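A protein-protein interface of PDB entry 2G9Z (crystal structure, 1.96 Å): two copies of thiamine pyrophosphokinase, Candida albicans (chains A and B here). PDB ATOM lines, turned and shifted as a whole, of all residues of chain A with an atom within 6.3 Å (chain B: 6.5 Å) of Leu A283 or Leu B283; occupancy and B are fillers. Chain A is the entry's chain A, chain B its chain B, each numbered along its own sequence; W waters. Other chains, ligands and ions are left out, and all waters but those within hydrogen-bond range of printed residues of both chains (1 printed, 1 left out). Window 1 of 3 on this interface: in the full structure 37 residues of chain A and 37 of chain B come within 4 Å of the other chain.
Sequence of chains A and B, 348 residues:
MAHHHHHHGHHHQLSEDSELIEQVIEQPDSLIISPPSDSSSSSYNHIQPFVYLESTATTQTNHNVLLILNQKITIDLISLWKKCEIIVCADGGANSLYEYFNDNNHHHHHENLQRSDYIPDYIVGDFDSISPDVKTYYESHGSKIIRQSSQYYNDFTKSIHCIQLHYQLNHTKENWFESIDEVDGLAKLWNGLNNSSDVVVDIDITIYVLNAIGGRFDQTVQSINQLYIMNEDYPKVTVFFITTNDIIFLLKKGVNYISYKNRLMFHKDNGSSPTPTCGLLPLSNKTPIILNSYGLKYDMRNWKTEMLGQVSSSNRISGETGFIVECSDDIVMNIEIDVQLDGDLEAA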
ATOM      1  N   PHE A 217      26.631 -10.875  15.910  1.00  0.00           N
ATOM      2  CA  PHE A 217      25.995 -11.851  15.033  1.00  0.00           C
ATOM      3  C   PHE A 217      25.989 -11.564  13.531  1.00  0.00           C
ATOM      4  O   PHE A 217      26.157 -12.488  12.729  1.00  0.00           O
ATOM      5  CB  PHE A 217      24.567 -12.122  15.503  1.00  0.00           C
ATOM      6  CG  PHE A 217      24.012 -13.409  14.994  1.00  0.00           C
ATOM      7  CD1 PHE A 217      24.654 -14.611  15.281  1.00  0.00           C
ATOM      8  CD2 PHE A 217      22.865 -13.431  14.214  1.00  0.00           C
ATOM      9  CE1 PHE A 217      24.155 -15.821  14.793  1.00  0.00           C
ATOM     10  CE2 PHE A 217      22.360 -14.636  13.722  1.00  0.00           C
ATOM     11  CZ  PHE A 217      23.008 -15.830  14.015  1.00  0.00           C
ATOM     12  N   VAL A 221      27.371 -14.055  10.579  1.00  0.00           N
ATOM     13  CA  VAL A 221      26.630 -14.435   9.394  1.00  0.00           C
ATOM     14  C   VAL A 221      27.340 -14.002   8.117  1.00  0.00           C
ATOM     15  O   VAL A 221      27.417 -14.772   7.157  1.00  0.00           O
ATOM     16  CB  VAL A 221      25.190 -13.869   9.441  1.00  0.00           C
ATOM     17  CG1 VAL A 221      24.475 -14.129   8.118  1.00  0.00           C
ATOM     18  CG2 VAL A 221      24.430 -14.534  10.583  1.00  0.00           C
ATOM     19  N   ILE A 224      30.119 -16.402   7.294  1.00  0.00           N
ATOM     20  CA  ILE A 224      29.625 -17.649   6.729  1.00  0.00           C
ATOM     21  C   ILE A 224      29.221 -17.379   5.279  1.00  0.00           C
ATOM     22  O   ILE A 224      29.527 -18.164   4.386  1.00  0.00           O
ATOM     23  CB  ILE A 224      28.411 -18.183   7.535  1.00  0.00           C
ATOM     24  CG1 ILE A 224      28.868 -18.587   8.945  1.00  0.00           C
ATOM     25  CG2 ILE A 224      27.761 -19.367   6.807  1.00  0.00           C
ATOM     26  CD1 ILE A 224      29.952 -19.665   8.981  1.00  0.00           C
ATOM     27  N   TYR A 228      30.775 -19.415   1.825  1.00  0.00           N
ATOM     28  CA  TYR A 228      30.053 -20.034   0.714  1.00  0.00           C
ATOM     29  C   TYR A 228      30.388 -19.378  -0.625  1.00  0.00           C
ATOM     30  O   TYR A 228      30.556 -20.062  -1.637  1.00  0.00           O
ATOM     31  CB  TYR A 228      28.542 -19.931   0.938  1.00  0.00           C
ATOM     32  CG  TYR A 228      27.947 -20.959   1.878  1.00  0.00           C
ATOM     33  CD1 TYR A 228      27.764 -22.285   1.472  1.00  0.00           C
ATOM     34  CD2 TYR A 228      27.510 -20.595   3.147  1.00  0.00           C
ATOM     35  CE1 TYR A 228      27.147 -23.217   2.312  1.00  0.00           C
ATOM     36  CE2 TYR A 228      26.896 -21.517   3.996  1.00  0.00           C
ATOM     37  CZ  TYR A 228      26.715 -22.823   3.568  1.00  0.00           C
ATOM     38  OH  TYR A 228      26.073 -23.717   4.384  1.00  0.00           O
ATOM     39  N   LEU A 281      25.579 -27.628   9.111  1.00  0.00           N
ATOM     40  CA  LEU A 281      24.681 -26.483   9.039  1.00  0.00           C
ATOM     41  C   LEU A 281      24.365 -25.970   7.640  1.00  0.00           C
ATOM     42  O   LEU A 281      25.216 -25.392   6.970  1.00  0.00           O
ATOM     43  CB  LEU A 281      25.291 -25.381   9.909  1.00  0.00           C
ATOM     44  CG  LEU A 281      25.986 -26.058  11.106  1.00  0.00           C
ATOM     45  CD1 LEU A 281      26.887 -25.092  11.832  1.00  0.00           C
ATOM     46  CD2 LEU A 281      24.939 -26.655  12.041  1.00  0.00           C
ATOM     47  N   PRO A 282      23.119 -26.177   7.186  1.00  0.00           N
ATOM     48  CA  PRO A 282      22.667 -25.744   5.860  1.00  0.00           C
ATOM     49  C   PRO A 282      22.346 -24.251   5.862  1.00  0.00           C
ATOM     50  O   PRO A 282      21.181 -23.853   5.909  1.00  0.00           O
ATOM     51  CB  PRO A 282      21.437 -26.612   5.627  1.00  0.00           C
ATOM     52  CG  PRO A 282      20.831 -26.689   6.994  1.00  0.00           C
ATOM     53  CD  PRO A 282      22.039 -26.879   7.910  1.00  0.00           C
ATOM     54  N   LEU A 283      23.390 -23.433   5.804  1.00  0.00           N
ATOM     55  CA  LEU A 283      23.238 -21.985   5.840  1.00  0.00           C
ATOM     56  C   LEU A 283      23.246 -21.267   4.488  1.00  0.00           C
ATOM     57  O   LEU A 283      23.287 -20.038   4.447  1.00  0.00           O
ATOM     58  CB  LEU A 283      24.320 -21.399   6.752  1.00  0.00           C
ATOM     59  CG  LEU A 283      24.177 -21.852   8.211  1.00  0.00           C
ATOM     60  CD1 LEU A 283      25.421 -21.518   9.021  1.00  0.00           C
ATOM     61  CD2 LEU A 283      22.947 -21.188   8.807  1.00  0.00           C
ATOM     62  N   SER A 284      23.198 -22.012   3.388  1.00  0.00           N
ATOM     63  CA  SER A 284      23.204 -21.385   2.063  1.00  0.00           C
ATOM     64  C   SER A 284      21.796 -21.222   1.488  1.00  0.00           C
ATOM     65  O   SER A 284      20.811 -21.585   2.120  1.00  0.00           O
ATOM     66  CB  SER A 284      24.035 -22.214   1.085  1.00  0.00           C
ATOM     67  OG  SER A 284      23.326 -23.373   0.688  1.00  0.00           O
ATOM     68  N   ASN A 285      21.721 -20.688   0.271  1.00  0.00           N
ATOM     69  CA  ASN A 285      20.449 -20.467  -0.405  1.00  0.00           C
ATOM     70  C   ASN A 285      20.056 -21.681  -1.247  1.00  0.00           C
ATOM     71  O   ASN A 285      19.146 -21.609  -2.073  1.00  0.00           O
ATOM     72  CB  ASN A 285      20.540 -19.215  -1.289  1.00  0.00           C
ATOM     73  CG  ASN A 285      21.447 -19.411  -2.488  1.00  0.00           C
ATOM     74  OD1 ASN A 285      22.352 -20.245  -2.470  1.00  0.00           O
ATOM     75  ND2 ASN A 285      21.219 -18.624  -3.535  1.00  0.00           N
ATOM     76  N   LYS A 286      20.757 -22.789  -1.041  1.00  0.00           N
ATOM     77  CA  LYS A 286      20.470 -24.025  -1.759  1.00  0.00           C
ATOM     78  C   LYS A 286      19.877 -25.006  -0.755  1.00  0.00           C
ATOM     79  O   LYS A 286      20.595 -25.574   0.071  1.00  0.00           O
ATOM     80  CB  LYS A 286      21.752 -24.601  -2.363  1.00  0.00           C
ATOM     81  CG  LYS A 286      22.404 -23.708  -3.411  1.00  0.00           C
ATOM     82  CD  LYS A 286      21.488 -23.498  -4.609  1.00  0.00           C
ATOM     83  CE  LYS A 286      22.159 -22.667  -5.693  1.00  0.00           C
ATOM     84  NZ  LYS A 286      22.491 -21.290  -5.232  1.00  0.00           N
ATOM     85  N   ILE A 289      19.408 -29.879   1.441  1.00  0.00           N
ATOM     86  CA  ILE A 289      20.643 -30.577   1.132  1.00  0.00           C
ATOM     87  C   ILE A 289      20.515 -32.017   1.614  1.00  0.00           C
ATOM     88  O   ILE A 289      20.118 -32.263   2.752  1.00  0.00           O
ATOM     89  CB  ILE A 289      21.844 -29.889   1.825  1.00  0.00           C
ATOM     90  CG1 ILE A 289      22.085 -28.522   1.177  1.00  0.00           C
ATOM     91  CG2 ILE A 289      23.083 -30.767   1.738  1.00  0.00           C
ATOM     92  CD1 ILE A 289      23.263 -27.769   1.733  1.00  0.00           C
ATOM     93  N   MET A 307      17.261 -25.070   6.891  1.00  0.00           N
ATOM     94  CA  MET A 307      16.795 -24.211   7.964  1.00  0.00           C
ATOM     95  C   MET A 307      15.276 -24.237   7.824  1.00  0.00           C
ATOM     96  O   MET A 307      14.761 -24.348   6.707  1.00  0.00           O
ATOM     97  CB  MET A 307      17.357 -22.794   7.798  1.00  0.00           C
ATOM     98  CG  MET A 307      18.861 -22.721   8.017  1.00  0.00           C
ATOM     99  SD  MET A 307      19.394 -23.337   9.648  1.00  0.00           S
ATOM    100  CE  MET A 307      19.242 -21.824  10.655  1.00  0.00           C
ATOM    101  N   LEU A 308      14.569 -24.154   8.947  1.00  0.00           N
ATOM    102  CA  LEU A 308      13.107 -24.230   8.955  1.00  0.00           C
ATOM    103  C   LEU A 308      12.740 -25.704   8.851  1.00  0.00           C
ATOM    104  O   LEU A 308      11.591 -26.058   8.606  1.00  0.00           O
ATOM    105  CB  LEU A 308      12.491 -23.473   7.774  1.00  0.00           C
ATOM    106  CG  LEU A 308      12.260 -21.969   7.890  1.00  0.00           C
ATOM    107  CD1 LEU A 308      11.023 -21.687   8.732  1.00  0.00           C
ATOM    108  CD2 LEU A 308      13.497 -21.327   8.476  1.00  0.00           C
ATOM    109  N   ASP A 330      27.139 -27.688  -1.216  1.00  0.00           N
ATOM    110  CA  ASP A 330      28.043 -27.234  -0.167  1.00  0.00           C
ATOM    111  C   ASP A 330      27.276 -27.054   1.137  1.00  0.00           C
ATOM    112  O   ASP A 330      26.122 -26.620   1.142  1.00  0.00           O
ATOM    113  CB  ASP A 330      28.702 -25.897  -0.534  1.00  0.00           C
ATOM    114  CG  ASP A 330      29.679 -26.008  -1.699  1.00  0.00           C
ATOM    115  OD1 ASP A 330      30.054 -27.138  -2.088  1.00  0.00           O
ATOM    116  OD2 ASP A 330      30.088 -24.947  -2.220  1.00  0.00           O
ATOM    117  N   ILE A 331      27.920 -27.400   2.243  1.00  0.00           N
ATOM    118  CA  ILE A 331      27.299 -27.241   3.543  1.00  0.00           C
ATOM    119  C   ILE A 331      28.379 -27.053   4.593  1.00  0.00           C
ATOM    120  O   ILE A 331      29.452 -27.659   4.527  1.00  0.00           O
ATOM    121  CB  ILE A 331      26.398 -28.458   3.901  1.00  0.00           C
ATOM    122  CG1 ILE A 331      25.659 -28.194   5.224  1.00  0.00           C
ATOM    123  CG2 ILE A 331      27.238 -29.726   3.986  1.00  0.00           C
ATOM    124  CD1 ILE A 331      24.607 -29.267   5.578  1.00  0.00           C
ATOM    125  N   VAL A 332      28.090 -26.192   5.555  1.00  0.00           N
ATOM    126  CA  VAL A 332      29.019 -25.892   6.631  1.00  0.00           C
ATOM    127  C   VAL A 332      29.074 -26.990   7.686  1.00  0.00           C
ATOM    128  O   VAL A 332      28.057 -27.581   8.035  1.00  0.00           O
ATOM    129  CB  VAL A 332      28.616 -24.583   7.353  1.00  0.00           C
ATOM    130  CG1 VAL A 332      29.427 -24.413   8.629  1.00  0.00           C
ATOM    131  CG2 VAL A 332      28.817 -23.395   6.423  1.00  0.00           C
ATOM    132  N   PHE B 217      29.136 -23.363  17.519  1.00  0.00           N
ATOM    133  CA  PHE B 217      28.409 -22.922  16.341  1.00  0.00           C
ATOM    134  C   PHE B 217      27.157 -23.713  15.966  1.00  0.00           C
ATOM    135  O   PHE B 217      26.152 -23.122  15.567  1.00  0.00           O
ATOM    136  CB  PHE B 217      29.349 -22.845  15.136  1.00  0.00           C
ATOM    137  CG  PHE B 217      28.815 -21.991  14.025  1.00  0.00           C
ATOM    138  CD1 PHE B 217      28.500 -20.654  14.256  1.00  0.00           C
ATOM    139  CD2 PHE B 217      28.606 -22.519  12.758  1.00  0.00           C
ATOM    140  CE1 PHE B 217      27.985 -19.857  13.240  1.00  0.00           C
ATOM    141  CE2 PHE B 217      28.091 -21.730  11.737  1.00  0.00           C
ATOM    142  CZ  PHE B 217      27.780 -20.396  11.981  1.00  0.00           C
ATOM    143  N   VAL B 221      23.342 -22.157  15.368  1.00  0.00           N
ATOM    144  CA  VAL B 221      22.502 -22.367  14.209  1.00  0.00           C
ATOM    145  C   VAL B 221      21.208 -23.085  14.567  1.00  0.00           C
ATOM    146  O   VAL B 221      20.150 -22.776  14.018  1.00  0.00           O
ATOM    147  CB  VAL B 221      23.270 -23.133  13.110  1.00  0.00           C
ATOM    148  CG1 VAL B 221      22.353 -23.446  11.945  1.00  0.00           C
ATOM    149  CG2 VAL B 221      24.443 -22.276  12.629  1.00  0.00           C
ATOM    150  N   ILE B 224      18.799 -20.541  15.919  1.00  0.00           N
ATOM    151  CA  ILE B 224      18.197 -19.712  14.886  1.00  0.00           C
ATOM    152  C   ILE B 224      17.155 -20.547  14.146  1.00  0.00           C
ATOM    153  O   ILE B 224      16.068 -20.066  13.827  1.00  0.00           O
ATOM    154  CB  ILE B 224      19.267 -19.199  13.898  1.00  0.00           C
ATOM    155  CG1 ILE B 224      20.202 -18.217  14.620  1.00  0.00           C
ATOM    156  CG2 ILE B 224      18.603 -18.513  12.705  1.00  0.00           C
ATOM    157  CD1 ILE B 224      19.507 -16.963  15.135  1.00  0.00           C
ATOM    158  N   TYR B 228      13.016 -19.582  13.691  1.00  0.00           N
ATOM    159  CA  TYR B 228      12.188 -19.536  12.494  1.00  0.00           C
ATOM    160  C   TYR B 228      11.026 -20.519  12.612  1.00  0.00           C
ATOM    161  O   TYR B 228       9.891 -20.197  12.264  1.00  0.00           O
ATOM    162  CB  TYR B 228      13.006 -19.902  11.256  1.00  0.00           C
ATOM    163  CG  TYR B 228      13.842 -18.784  10.667  1.00  0.00           C
ATOM    164  CD1 TYR B 228      13.248 -17.730   9.965  1.00  0.00           C
ATOM    165  CD2 TYR B 228      15.229 -18.807  10.765  1.00  0.00           C
ATOM    166  CE1 TYR B 228      14.029 -16.726   9.364  1.00  0.00           C
ATOM    167  CE2 TYR B 228      16.017 -17.815  10.172  1.00  0.00           C
ATOM    168  CZ  TYR B 228      15.412 -16.782   9.470  1.00  0.00           C
ATOM    169  OH  TYR B 228      16.199 -15.835   8.849  1.00  0.00           O
ATOM    170  N   LEU B 281      19.654 -10.753   8.596  1.00  0.00           N
ATOM    171  CA  LEU B 281      20.230 -12.028   8.184  1.00  0.00           C
ATOM    172  C   LEU B 281      19.238 -13.059   7.658  1.00  0.00           C
ATOM    173  O   LEU B 281      18.441 -13.615   8.410  1.00  0.00           O
ATOM    174  CB  LEU B 281      21.022 -12.578   9.377  1.00  0.00           C
ATOM    175  CG  LEU B 281      21.668 -11.400  10.133  1.00  0.00           C
ATOM    176  CD1 LEU B 281      22.146 -11.826  11.500  1.00  0.00           C
ATOM    177  CD2 LEU B 281      22.815 -10.819   9.309  1.00  0.00           C
ATOM    178  N   PRO B 282      19.291 -13.334   6.345  1.00  0.00           N
ATOM    179  CA  PRO B 282      18.407 -14.294   5.678  1.00  0.00           C
ATOM    180  C   PRO B 282      18.907 -15.719   5.899  1.00  0.00           C
ATOM    181  O   PRO B 282      19.539 -16.313   5.031  1.00  0.00           O
ATOM    182  CB  PRO B 282      18.489 -13.858   4.222  1.00  0.00           C
ATOM    183  CG  PRO B 282      19.922 -13.473   4.087  1.00  0.00           C
ATOM    184  CD  PRO B 282      20.220 -12.715   5.378  1.00  0.00           C
ATOM    185  N   LEU B 283      18.624 -16.259   7.075  1.00  0.00           N
ATOM    186  CA  LEU B 283      19.084 -17.592   7.421  1.00  0.00           C
ATOM    187  C   LEU B 283      18.082 -18.726   7.216  1.00  0.00           C
ATOM    188  O   LEU B 283      18.375 -19.875   7.552  1.00  0.00           O
ATOM    189  CB  LEU B 283      19.571 -17.586   8.866  1.00  0.00           C
ATOM    190  CG  LEU B 283      20.796 -16.696   9.083  1.00  0.00           C
ATOM    191  CD1 LEU B 283      21.042 -16.477  10.565  1.00  0.00           C
ATOM    192  CD2 LEU B 283      22.000 -17.343   8.420  1.00  0.00           C
ATOM    193  N   SER B 284      16.910 -18.424   6.668  1.00  0.00           N
ATOM    194  CA  SER B 284      15.905 -19.466   6.454  1.00  0.00           C
ATOM    195  C   SER B 284      16.020 -20.097   5.072  1.00  0.00           C
ATOM    196  O   SER B 284      16.859 -19.704   4.266  1.00  0.00           O
ATOM    197  CB  SER B 284      14.500 -18.895   6.615  1.00  0.00           C
ATOM    198  OG  SER B 284      14.150 -18.131   5.478  1.00  0.00           O
ATOM    199  N   ASN B 285      15.150 -21.065   4.799  1.00  0.00           N
ATOM    200  CA  ASN B 285      15.152 -21.759   3.519  1.00  0.00           C
ATOM    201  C   ASN B 285      14.312 -21.007   2.484  1.00  0.00           C
ATOM    202  O   ASN B 285      14.132 -21.475   1.361  1.00  0.00           O
ATOM    203  CB  ASN B 285      14.621 -23.189   3.696  1.00  0.00           C
ATOM    204  CG  ASN B 285      13.110 -23.244   3.781  1.00  0.00           C
ATOM    205  OD1 ASN B 285      12.487 -22.514   4.554  1.00  0.00           O
ATOM    206  ND2 ASN B 285      12.510 -24.121   2.984  1.00  0.00           N
ATOM    207  N   LYS B 286      13.789 -19.847   2.869  1.00  0.00           N
ATOM    208  CA  LYS B 286      12.992 -19.031   1.957  1.00  0.00           C
ATOM    209  C   LYS B 286      13.918 -17.959   1.399  1.00  0.00           C
ATOM    210  O   LYS B 286      14.328 -17.046   2.115  1.00  0.00           O
ATOM    211  CB  LYS B 286      11.820 -18.383   2.697  1.00  0.00           C
ATOM    212  CG  LYS B 286      10.826 -19.379   3.271  1.00  0.00           C
ATOM    213  CD  LYS B 286       9.744 -18.680   4.080  1.00  0.00           C
ATOM    214  CE  LYS B 286       8.789 -19.681   4.714  1.00  0.00           C
ATOM    215  NZ  LYS B 286       8.056 -20.477   3.691  1.00  0.00           N
ATOM    216  N   ILE B 289      14.956 -12.837  -0.145  1.00  0.00           N
ATOM    217  CA  ILE B 289      14.021 -12.021   0.604  1.00  0.00           C
ATOM    218  C   ILE B 289      14.151 -10.576   0.133  1.00  0.00           C
ATOM    219  O   ILE B 289      15.261 -10.068  -0.019  1.00  0.00           O
ATOM    220  CB  ILE B 289      14.296 -12.124   2.123  1.00  0.00           C
ATOM    221  CG1 ILE B 289      13.974 -13.547   2.597  1.00  0.00           C
ATOM    222  CG2 ILE B 289      13.465 -11.100   2.882  1.00  0.00           C
ATOM    223  CD1 ILE B 289      14.095 -13.762   4.081  1.00  0.00           C
ATOM    224  N   MET B 307      21.724 -15.801   1.459  1.00  0.00           N
ATOM    225  CA  MET B 307      23.064 -16.318   1.692  1.00  0.00           C
ATOM    226  C   MET B 307      23.568 -16.672   0.300  1.00  0.00           C
ATOM    227  O   MET B 307      22.780 -17.058  -0.562  1.00  0.00           O
ATOM    228  CB  MET B 307      23.021 -17.547   2.600  1.00  0.00           C
ATOM    229  CG  MET B 307      22.626 -17.229   4.033  1.00  0.00           C
ATOM    230  SD  MET B 307      23.696 -15.975   4.812  1.00  0.00           S
ATOM    231  CE  MET B 307      25.087 -16.977   5.344  1.00  0.00           C
ATOM    232  N   LEU B 308      24.873 -16.527   0.091  1.00  0.00           N
ATOM    233  CA  LEU B 308      25.501 -16.753  -1.210  1.00  0.00           C
ATOM    234  C   LEU B 308      25.176 -15.567  -2.103  1.00  0.00           C
ATOM    235  O   LEU B 308      25.334 -15.625  -3.319  1.00  0.00           O
ATOM    236  CB  LEU B 308      25.020 -18.044  -1.882  1.00  0.00           C
ATOM    237  CG  LEU B 308      25.908 -19.239  -1.553  1.00  0.00           C
ATOM    238  CD1 LEU B 308      25.532 -19.730  -0.175  1.00  0.00           C
ATOM    239  CD2 LEU B 308      25.752 -20.347  -2.586  1.00  0.00           C
ATOM    240  N   ASP B 330       9.914 -13.933   6.650  1.00  0.00           N
ATOM    241  CA  ASP B 330      10.582 -13.786   7.937  1.00  0.00           C
ATOM    242  C   ASP B 330      12.088 -13.676   7.745  1.00  0.00           C
ATOM    243  O   ASP B 330      12.673 -14.364   6.901  1.00  0.00           O
ATOM    244  CB  ASP B 330      10.304 -14.988   8.846  1.00  0.00           C
ATOM    245  CG  ASP B 330       8.844 -15.103   9.251  1.00  0.00           C
ATOM    246  OD1 ASP B 330       8.061 -14.170   8.977  1.00  0.00           O
ATOM    247  OD2 ASP B 330       8.484 -16.134   9.860  1.00  0.00           O
ATOM    248  N   ILE B 331      12.713 -12.800   8.520  1.00  0.00           N
ATOM    249  CA  ILE B 331      14.155 -12.645   8.454  1.00  0.00           C
ATOM    250  C   ILE B 331      14.670 -12.226   9.821  1.00  0.00           C
ATOM    251  O   ILE B 331      14.003 -11.495  10.560  1.00  0.00           O
ATOM    252  CB  ILE B 331      14.584 -11.608   7.384  1.00  0.00           C
ATOM    253  CG1 ILE B 331      16.115 -11.590   7.272  1.00  0.00           C
ATOM    254  CG2 ILE B 331      14.056 -10.221   7.748  1.00  0.00           C
ATOM    255  CD1 ILE B 331      16.639 -10.827   6.051  1.00  0.00           C
ATOM    256  N   VAL B 332      15.850 -12.725  10.159  1.00  0.00           N
ATOM    257  CA  VAL B 332      16.476 -12.434  11.434  1.00  0.00           C
ATOM    258  C   VAL B 332      17.116 -11.051  11.433  1.00  0.00           C
ATOM    259  O   VAL B 332      17.694 -10.632  10.436  1.00  0.00           O
ATOM    260  CB  VAL B 332      17.600 -13.454  11.752  1.00  0.00           C
ATOM    261  CG1 VAL B 332      18.400 -12.993  12.974  1.00  0.00           C
ATOM    262  CG2 VAL B 332      17.005 -14.832  11.985  1.00  0.00           C
HETATM  263  O   HOH W   1      18.431 -20.996   2.861  1.00  0.00           O
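O of Leu B281 sits at hydrogen-bond distance from OH of Tyr B228.
The side-chain amide oxygen (OD1) of Asn A285 sits at hydrogen-bond distance from the side-chain amino group (NZ) of Lys A286, at 3.0 Å.
N of Leu B283 lies within hydrogen-bond range of OH of Tyr B228 (3.0 Å).
The side-chain hydroxyl (OH) of Tyr B228 lies within hydrogen-bond range of the backbone NH (N) of Ser B284 (3.5 Å).
OG of Ser B284 is in hydrogen-bond range of N of Lys B286 (3.1 Å).
The backbone NH of Leu B281 is in hydrogen-bond range of the backbone carbonyl oxygen of Val B332 (2.7 Å).
Among the printed residues, pairs that only touch across the chains: Leu A283 with Met B307, Met A307 with Leu B283, Ser A284 with Leu B308, Leu A308 with Tyr B228, Asn A285 with Met B307, Tyr A228 with Leu B308, Leu A308 with Ser B284, Met A307 with Asn B285, Leu A281 with Phe B217, Phe A217 with Leu B281, Leu A308 with Asn B285, Asn A285 with Leu B308, Met A307 with Val B221, Val A221 with Leu B281, Val A221 with Met B307, Ile A224 with Phe B217, Phe A217 with Ile B224, Leu A281 with Val B221, Leu A283 with Val B221, Leu A283 with Phe B217, Met A307 with Ser B284, Ile A224 with Met B307, Ser A284 with Met B307, Phe A217 with Leu B283, Val A221 with Leu B283, Met A307 with Ile B224 and Leu A283 with Leu B283.
Of the printed residues of chain B, Phe A217 touches Ile B224, Leu B281 and Leu B283.
Printed residues of chain B within 4 Å of Ile A224: Phe B217 (3.7 Å) and Met B307 (3.9 Å).
Leu A283 touches just these residues of chain B: Phe B217 (3.8 Å), Val B221 (3.8 Å), Leu B283 (3.98 Å) and Met B307 (2.9 Å).
Lys A286 touches none of the printed residues of chain B.
Of the printed residues of chain A, Ile B224 touches Phe A217 (3.7 Å) and Met A307 (3.9 Å).
The nearest residue of chain B that does not touch Leu A283 is Leu B308 (5.1 Å).
The nearest residue of chain A that does not touch Leu B283 is Pro A282 (5.1 Å).
Of the 16 printed residues of chain B, 10 touch a printed residue of chain A.
Printed residues of chain B that touch a printed residue of chain A: Phe B217, Val B221, Ile B224, Tyr B228, Leu B281, Leu B283, Ser B284, Asn B285, Met B307 and Leu B308.
Of the 16 printed residues of chain A, 10 touch a printed residue of chain B.
Hydrophobic or aromatic side chains of chain A within 4 Å of the printed part of chain B: Phe A217, Val A221, Ile A224, Tyr A228, Leu A281, Leu A283, Met A307 and Leu A308.
Among the printed residues, no Asp or Glu carboxylate lies within 4 Å of a Lys or Arg side-chain nitrogen of the other chain.
Phe A217 touches Ile B224, and with the chains exchanged Ile A224 touches Phe B217.
Tyr A228 touches Leu B308, and with the chains exchanged Leu A308 touches Tyr B228.
Ser A284 touches Met B307, and with the chains exchanged Met A307 touches Ser B284.
Asn A285 touches Leu B308, and with the chains exchanged Leu A308 touches Asn B285.
16 positions are printed for both chains.
Water W1 bridges O of Ser B284 and O of Ser A284.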
